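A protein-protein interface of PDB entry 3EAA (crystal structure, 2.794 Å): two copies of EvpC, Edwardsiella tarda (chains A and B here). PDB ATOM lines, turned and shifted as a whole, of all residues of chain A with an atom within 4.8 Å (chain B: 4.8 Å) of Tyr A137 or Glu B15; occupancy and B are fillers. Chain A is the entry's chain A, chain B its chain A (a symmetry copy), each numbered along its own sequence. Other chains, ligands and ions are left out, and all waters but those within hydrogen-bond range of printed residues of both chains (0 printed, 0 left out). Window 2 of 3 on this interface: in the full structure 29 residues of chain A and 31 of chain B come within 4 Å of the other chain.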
ATOM      1  N   PHE A  97     -30.089  -2.248  10.049  1.00  0.00           N
ATOM      2  CA  PHE A  97     -29.967  -2.025   8.621  1.00  0.00           C
ATOM      3  C   PHE A  97     -30.856  -2.991   7.882  1.00  0.00           C
ATOM      4  O   PHE A  97     -30.896  -3.012   6.657  1.00  0.00           O
ATOM      5  CB  PHE A  97     -28.516  -2.188   8.179  1.00  0.00           C
ATOM      6  CG  PHE A  97     -27.913  -3.490   8.581  1.00  0.00           C
ATOM      7  CD1 PHE A  97     -27.913  -4.560   7.715  1.00  0.00           C
ATOM      8  CD2 PHE A  97     -27.354  -3.651   9.833  1.00  0.00           C
ATOM      9  CE1 PHE A  97     -27.358  -5.762   8.085  1.00  0.00           C
ATOM     10  CE2 PHE A  97     -26.798  -4.859  10.214  1.00  0.00           C
ATOM     11  CZ  PHE A  97     -26.802  -5.911   9.337  1.00  0.00           C
ATOM     12  N   CYS A  98     -31.580  -3.796   8.637  1.00  0.00           N
ATOM     13  CA  CYS A  98     -32.507  -4.738   8.040  1.00  0.00           C
ATOM     14  C   CYS A  98     -33.596  -5.084   9.022  1.00  0.00           C
ATOM     15  O   CYS A  98     -33.329  -5.637  10.084  1.00  0.00           O
ATOM     16  CB  CYS A  98     -31.786  -6.014   7.628  1.00  0.00           C
ATOM     17  SG  CYS A  98     -32.883  -7.180   6.824  1.00  0.00           S
ATOM     18  N   TRP A 135     -39.651  -6.798   4.197  1.00  0.00           N
ATOM     19  CA  TRP A 135     -38.184  -6.742   4.198  1.00  0.00           C
ATOM     20  C   TRP A 135     -37.578  -5.541   4.930  1.00  0.00           C
ATOM     21  O   TRP A 135     -37.031  -5.697   6.015  1.00  0.00           O
ATOM     22  CB  TRP A 135     -37.574  -6.818   2.793  1.00  0.00           C
ATOM     23  CG  TRP A 135     -38.415  -7.418   1.723  1.00  0.00           C
ATOM     24  CD1 TRP A 135     -38.637  -6.894   0.485  1.00  0.00           C
ATOM     25  CD2 TRP A 135     -39.134  -8.652   1.774  1.00  0.00           C
ATOM     26  NE1 TRP A 135     -39.453  -7.721  -0.238  1.00  0.00           N
ATOM     27  CE2 TRP A 135     -39.773  -8.802   0.524  1.00  0.00           C
ATOM     28  CE3 TRP A 135     -39.299  -9.637   2.744  1.00  0.00           C
ATOM     29  CZ2 TRP A 135     -40.571  -9.910   0.227  1.00  0.00           C
ATOM     30  CZ3 TRP A 135     -40.096 -10.740   2.441  1.00  0.00           C
ATOM     31  CH2 TRP A 135     -40.719 -10.862   1.192  1.00  0.00           C
ATOM     32  N   GLU A 136     -37.642  -4.361   4.318  1.00  0.00           N
ATOM     33  CA  GLU A 136     -37.011  -3.156   4.882  1.00  0.00           C
ATOM     34  C   GLU A 136     -35.504  -3.285   5.085  1.00  0.00           C
ATOM     35  O   GLU A 136     -35.026  -4.094   5.885  1.00  0.00           O
ATOM     36  CB  GLU A 136     -37.644  -2.759   6.212  1.00  0.00           C
ATOM     37  CG  GLU A 136     -39.102  -2.381   6.157  1.00  0.00           C
ATOM     38  CD  GLU A 136     -39.558  -1.738   7.448  1.00  0.00           C
ATOM     39  OE1 GLU A 136     -38.685  -1.300   8.224  1.00  0.00           O
ATOM     40  OE2 GLU A 136     -40.781  -1.660   7.690  1.00  0.00           O
ATOM     41  N   TYR A 137     -34.767  -2.454   4.366  1.00  0.00           N
ATOM     42  CA  TYR A 137     -33.320  -2.384   4.472  1.00  0.00           C
ATOM     43  C   TYR A 137     -32.894  -0.923   4.622  1.00  0.00           C
ATOM     44  O   TYR A 137     -33.580  -0.016   4.152  1.00  0.00           O
ATOM     45  CB  TYR A 137     -32.693  -2.953   3.205  1.00  0.00           C
ATOM     46  CG  TYR A 137     -31.195  -2.731   3.083  1.00  0.00           C
ATOM     47  CD1 TYR A 137     -30.302  -3.619   3.664  1.00  0.00           C
ATOM     48  CD2 TYR A 137     -30.677  -1.649   2.374  1.00  0.00           C
ATOM     49  CE1 TYR A 137     -28.941  -3.440   3.558  1.00  0.00           C
ATOM     50  CE2 TYR A 137     -29.311  -1.459   2.262  1.00  0.00           C
ATOM     51  CZ  TYR A 137     -28.443  -2.364   2.857  1.00  0.00           C
ATOM     52  OH  TYR A 137     -27.071  -2.206   2.768  1.00  0.00           O
ATOM     53  N   VAL A 138     -31.755  -0.699   5.264  1.00  0.00           N
ATOM     54  CA  VAL A 138     -31.212   0.644   5.408  1.00  0.00           C
ATOM     55  C   VAL A 138     -29.712   0.639   5.150  1.00  0.00           C
ATOM     56  O   VAL A 138     -28.971  -0.057   5.841  1.00  0.00           O
ATOM     57  CB  VAL A 138     -31.467   1.197   6.824  1.00  0.00           C
ATOM     58  CG1 VAL A 138     -30.728   2.495   7.034  1.00  0.00           C
ATOM     59  CG2 VAL A 138     -32.954   1.397   7.061  1.00  0.00           C
ATOM     60  N   PRO A 139     -29.257   1.413   4.149  1.00  0.00           N
ATOM     61  CA  PRO A 139     -27.840   1.651   3.850  1.00  0.00           C
ATOM     62  C   PRO A 139     -27.131   2.368   4.996  1.00  0.00           C
ATOM     63  O   PRO A 139     -27.786   2.824   5.936  1.00  0.00           O
ATOM     64  CB  PRO A 139     -27.901   2.577   2.634  1.00  0.00           C
ATOM     65  CG  PRO A 139     -29.265   3.153   2.685  1.00  0.00           C
ATOM     66  CD  PRO A 139     -30.109   2.021   3.122  1.00  0.00           C
ATOM     67  N   GLY A 148     -30.947   6.824   3.766  1.00  0.00           N
ATOM     68  CA  GLY A 148     -32.372   6.638   3.577  1.00  0.00           C
ATOM     69  C   GLY A 148     -32.790   5.183   3.656  1.00  0.00           C
ATOM     70  O   GLY A 148     -32.041   4.290   3.279  1.00  0.00           O
ATOM     71  N   LYS A 149     -33.993   4.938   4.154  1.00  0.00           N
ATOM     72  CA  LYS A 149     -34.511   3.577   4.238  1.00  0.00           C
ATOM     73  C   LYS A 149     -35.078   3.106   2.905  1.00  0.00           C
ATOM     74  O   LYS A 149     -35.729   3.872   2.197  1.00  0.00           O
ATOM     75  CB  LYS A 149     -35.577   3.453   5.328  1.00  0.00           C
ATOM     76  CG  LYS A 149     -36.059   2.028   5.523  1.00  0.00           C
ATOM     77  CD  LYS A 149     -37.165   1.942   6.564  1.00  0.00           C
ATOM     78  CE  LYS A 149     -36.620   1.968   7.984  1.00  0.00           C
ATOM     79  NZ  LYS A 149     -37.709   1.711   8.970  1.00  0.00           N
ATOM     80  N   ILE A 150     -34.841   1.838   2.576  1.00  0.00           N
ATOM     81  CA  ILE A 150     -35.245   1.307   1.279  1.00  0.00           C
ATOM     82  C   ILE A 150     -36.617   0.645   1.306  1.00  0.00           C
ATOM     83  O   ILE A 150     -36.773  -0.469   1.810  1.00  0.00           O
ATOM     84  CB  ILE A 150     -34.206   0.337   0.693  1.00  0.00           C
ATOM     85  CG1 ILE A 150     -32.840   1.024   0.594  1.00  0.00           C
ATOM     86  CG2 ILE A 150     -34.654  -0.160  -0.682  1.00  0.00           C
ATOM     87  CD1 ILE A 150     -32.894   2.443   0.055  1.00  0.00           C
ATOM     88  N   ASP B  13     -31.001  -0.244  -8.576  1.00  0.00           N
ATOM     89  CA  ASP B  13     -29.702   0.236  -8.114  1.00  0.00           C
ATOM     90  C   ASP B  13     -29.075  -0.647  -7.048  1.00  0.00           C
ATOM     91  O   ASP B  13     -29.630  -0.822  -5.967  1.00  0.00           O
ATOM     92  CB  ASP B  13     -29.806   1.666  -7.575  1.00  0.00           C
ATOM     93  CG  ASP B  13     -30.398   2.626  -8.577  1.00  0.00           C
ATOM     94  OD1 ASP B  13     -30.002   2.562  -9.757  1.00  0.00           O
ATOM     95  OD2 ASP B  13     -31.258   3.443  -8.189  1.00  0.00           O
ATOM     96  N   GLY B  14     -27.898  -1.177  -7.353  1.00  0.00           N
ATOM     97  CA  GLY B  14     -27.088  -1.841  -6.355  1.00  0.00           C
ATOM     98  C   GLY B  14     -26.262  -0.799  -5.632  1.00  0.00           C
ATOM     99  O   GLY B  14     -26.685   0.350  -5.516  1.00  0.00           O
ATOM    100  N   GLU B  15     -25.074  -1.177  -5.178  1.00  0.00           N
ATOM    101  CA  GLU B  15     -24.298  -0.330  -4.284  1.00  0.00           C
ATOM    102  C   GLU B  15     -22.858  -0.072  -4.744  1.00  0.00           C
ATOM    103  O   GLU B  15     -22.100   0.607  -4.059  1.00  0.00           O
ATOM    104  CB  GLU B  15     -24.279  -0.983  -2.900  1.00  0.00           C
ATOM    105  CG  GLU B  15     -24.293  -0.037  -1.724  1.00  0.00           C
ATOM    106  CD  GLU B  15     -25.011  -0.641  -0.543  1.00  0.00           C
ATOM    107  OE1 GLU B  15     -24.387  -0.778   0.528  1.00  0.00           O
ATOM    108  OE2 GLU B  15     -26.204  -0.990  -0.696  1.00  0.00           O
ATOM    109  N   SER B  16     -22.470  -0.607  -5.895  1.00  0.00           N
ATOM    110  CA  SER B  16     -21.075  -0.496  -6.317  1.00  0.00           C
ATOM    111  C   SER B  16     -20.585   0.949  -6.399  1.00  0.00           C
ATOM    112  O   SER B  16     -21.366   1.896  -6.336  1.00  0.00           O
ATOM    113  CB  SER B  16     -20.823  -1.209  -7.645  1.00  0.00           C
ATOM    114  OG  SER B  16     -19.457  -1.095  -7.998  1.00  0.00           O
ATOM    115  N   THR B  17     -19.279   1.103  -6.554  1.00  0.00           N
ATOM    116  CA  THR B  17     -18.668   2.414  -6.475  1.00  0.00           C
ATOM    117  C   THR B  17     -17.651   2.674  -7.573  1.00  0.00           C
ATOM    118  O   THR B  17     -17.438   3.828  -7.949  1.00  0.00           O
ATOM    119  CB  THR B  17     -17.960   2.599  -5.139  1.00  0.00           C
ATOM    120  OG1 THR B  17     -18.780   2.074  -4.090  1.00  0.00           O
ATOM    121  CG2 THR B  17     -17.682   4.076  -4.893  1.00  0.00           C
ATOM    122  N   LYS B  23     -23.230   2.216  -8.969  1.00  0.00           N
ATOM    123  CA  LYS B  23     -24.516   1.734  -8.462  1.00  0.00           C
ATOM    124  C   LYS B  23     -24.898   0.329  -8.963  1.00  0.00           C
ATOM    125  O   LYS B  23     -26.012  -0.149  -8.730  1.00  0.00           O
ATOM    126  CB  LYS B  23     -25.630   2.750  -8.747  1.00  0.00           C
ATOM    127  CG  LYS B  23     -25.567   3.992  -7.861  1.00  0.00           C
ATOM    128  CD  LYS B  23     -26.379   5.166  -8.420  1.00  0.00           C
ATOM    129  CE  LYS B  23     -27.757   5.290  -7.771  1.00  0.00           C
ATOM    130  NZ  LYS B  23     -28.331   6.662  -7.921  1.00  0.00           N
ATOM    131  N   TRP B  24     -23.968  -0.331  -9.646  1.00  0.00           N
ATOM    132  CA  TRP B  24     -24.141  -1.728 -10.008  1.00  0.00           C
ATOM    133  C   TRP B  24     -24.185  -2.557  -8.745  1.00  0.00           C
ATOM    134  O   TRP B  24     -23.845  -2.066  -7.673  1.00  0.00           O
ATOM    135  CB  TRP B  24     -22.955  -2.198 -10.834  1.00  0.00           C
ATOM    136  CG  TRP B  24     -23.035  -1.846 -12.261  1.00  0.00           C
ATOM    137  CD1 TRP B  24     -23.192  -0.603 -12.788  1.00  0.00           C
ATOM    138  CD2 TRP B  24     -22.936  -2.746 -13.367  1.00  0.00           C
ATOM    139  NE1 TRP B  24     -23.209  -0.673 -14.157  1.00  0.00           N
ATOM    140  CE2 TRP B  24     -23.053  -1.977 -14.538  1.00  0.00           C
ATOM    141  CE3 TRP B  24     -22.767  -4.132 -13.478  1.00  0.00           C
ATOM    142  CZ2 TRP B  24     -23.003  -2.544 -15.809  1.00  0.00           C
ATOM    143  CZ3 TRP B  24     -22.718  -4.693 -14.742  1.00  0.00           C
ATOM    144  CH2 TRP B  24     -22.835  -3.900 -15.889  1.00  0.00           C
ATOM    145  N   ILE B  25     -24.574  -3.822  -8.874  1.00  0.00           N
ATOM    146  CA  ILE B  25     -24.546  -4.742  -7.745  1.00  0.00           C
ATOM    147  C   ILE B  25     -23.233  -5.516  -7.716  1.00  0.00           C
ATOM    148  O   ILE B  25     -22.907  -6.223  -8.666  1.00  0.00           O
ATOM    149  CB  ILE B  25     -25.695  -5.770  -7.805  1.00  0.00           C
ATOM    150  CG1 ILE B  25     -27.055  -5.102  -7.585  1.00  0.00           C
ATOM    151  CG2 ILE B  25     -25.466  -6.883  -6.789  1.00  0.00           C
ATOM    152  CD1 ILE B  25     -27.654  -4.514  -8.860  1.00  0.00           C
ATOM    153  N   MET B  63     -25.844  -8.436   1.497  1.00  0.00           N
ATOM    154  CA  MET B  63     -27.014  -7.585   1.503  1.00  0.00           C
ATOM    155  C   MET B  63     -26.605  -6.206   1.061  1.00  0.00           C
ATOM    156  O   MET B  63     -25.579  -5.670   1.483  1.00  0.00           O
ATOM    157  CB  MET B  63     -27.611  -7.486   2.901  1.00  0.00           C
ATOM    158  CG  MET B  63     -28.773  -8.426   3.143  1.00  0.00           C
ATOM    159  SD  MET B  63     -29.933  -7.798   4.580  1.00  0.00           S
ATOM    160  CE  MET B  63     -31.474  -8.946   4.205  1.00  0.00           C
ATOM    161  N   ASP B  64     -27.418  -5.613   0.215  1.00  0.00           N
ATOM    162  CA  ASP B  64     -27.206  -4.226  -0.117  1.00  0.00           C
ATOM    163  C   ASP B  64     -28.548  -3.548  -0.292  1.00  0.00           C
ATOM    164  O   ASP B  64     -29.541  -3.928   0.325  1.00  0.00           O
ATOM    165  CB  ASP B  64     -26.351  -4.106  -1.372  1.00  0.00           C
ATOM    166  CG  ASP B  64     -26.662  -5.173  -2.370  1.00  0.00           C
ATOM    167  OD1 ASP B  64     -27.862  -5.375  -2.638  1.00  0.00           O
ATOM    168  OD2 ASP B  64     -25.717  -5.806  -2.882  1.00  0.00           O
ATOM    169  N   CYS B  65     -28.559  -2.536  -1.139  1.00  0.00           N
ATOM    170  CA  CYS B  65     -29.740  -1.740  -1.380  1.00  0.00           C
ATOM    171  C   CYS B  65     -30.633  -2.440  -2.386  1.00  0.00           C
ATOM    172  O   CYS B  65     -31.758  -2.010  -2.632  1.00  0.00           O
ATOM    173  CB  CYS B  65     -29.315  -0.397  -1.947  1.00  0.00           C
ATOM    174  SG  CYS B  65     -28.136  -0.582  -3.281  1.00  0.00           S
ATOM    175  N   SER B  67     -31.236  -5.763  -2.230  1.00  0.00           N
ATOM    176  CA  SER B  67     -31.891  -6.842  -1.512  1.00  0.00           C
ATOM    177  C   SER B  67     -33.402  -6.753  -1.615  1.00  0.00           C
ATOM    178  O   SER B  67     -34.041  -7.625  -2.199  1.00  0.00           O
ATOM    179  CB  SER B  67     -31.483  -6.822  -0.046  1.00  0.00           C
ATOM    180  OG  SER B  67     -30.081  -6.727   0.067  1.00  0.00           O
ATOM    181  N   VAL B  68     -33.969  -5.689  -1.056  1.00  0.00           N
ATOM    182  CA  VAL B  68     -35.417  -5.584  -0.956  1.00  0.00           C
ATOM    183  C   VAL B  68     -36.093  -5.786  -2.304  1.00  0.00           C
ATOM    184  O   VAL B  68     -37.113  -6.466  -2.397  1.00  0.00           O
ATOM    185  CB  VAL B  68     -35.858  -4.261  -0.329  1.00  0.00           C
ATOM    186  CG1 VAL B  68     -37.365  -4.109  -0.435  1.00  0.00           C
ATOM    187  CG2 VAL B  68     -35.433  -4.209   1.124  1.00  0.00           C
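SG of Cys A98 lies close to SD of Met B63 (3.8 Å). The indole nitrogen (NE1) of Trp A135 sits close to the backbone carbonyl oxygen (O) of Val B68 (3.4 Å).
The backbone carbonyl oxygen (O) of Asp B13 sits at hydrogen-bond distance from the side-chain sulfur (SG) of Cys B65, at 3.1 Å. The backbone carbonyl oxygen (O) of Gly B14 is in hydrogen-bond range of the side-chain sulfur (SG) of Cys B65. The backbone carbonyl oxygen of Tyr A137 is in hydrogen-bond range of the backbone NH of Ile A150. The backbone NH (N) of Glu B15 lies within hydrogen-bond range of the backbone carbonyl oxygen (O) of Trp B24 (2.9 Å). The backbone NH (N) of Cys B65 sits at hydrogen-bond distance from the side-chain carboxylate (OE2) of Glu B15 (2.9 Å). The side-chain carboxylate (OE1) of Glu A136 lies within salt-bridge range of the side-chain amino group (NZ) of Lys A149.
Among the printed residues, pairs that only touch across the chains: Glu A136 with Val B68 (3.9 Å), Tyr A137 with Glu B15 (3.8 Å), Tyr A137 with Met B63 (3.98 Å), Tyr A137 with Asp B64 (3.1 Å), Tyr A137 with Cys B65 (3.6 Å), Tyr A137 with Val B68 (3.7 Å) and Ile A150 with Cys B65 (3.95 Å).
Of the printed residues of chain B, Trp A135 touches Val B68. Gly B14 touches none of the printed residues of chain A. Of the printed residues of chain A, Glu B15 touches Tyr A137. Trp B24 touches none of the printed residues of chain A. Of the printed residues of chain A, Cys B65 touches Tyr A137 (3.6 Å) and Ile A150 (3.95 Å). The nearest printed residue of chain B that does not touch Tyr A137 is Ser B67 (4.8 Å). The nearest printed residue of chain A that does not touch Glu B15 is Pro A139 (5.2 Å). The nearest printed residue of chain B that does not touch Cys A98 is Val B68 (6.9 Å).
Of the 10 printed residues of chain A, 5 touch a printed residue of chain B. Of the 13 printed residues of chain B, 5 touch a printed residue of chain A. Along chain B the printed residues that touch a printed residue of chain A span positions 15 to 68.
No position is printed for both chains.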
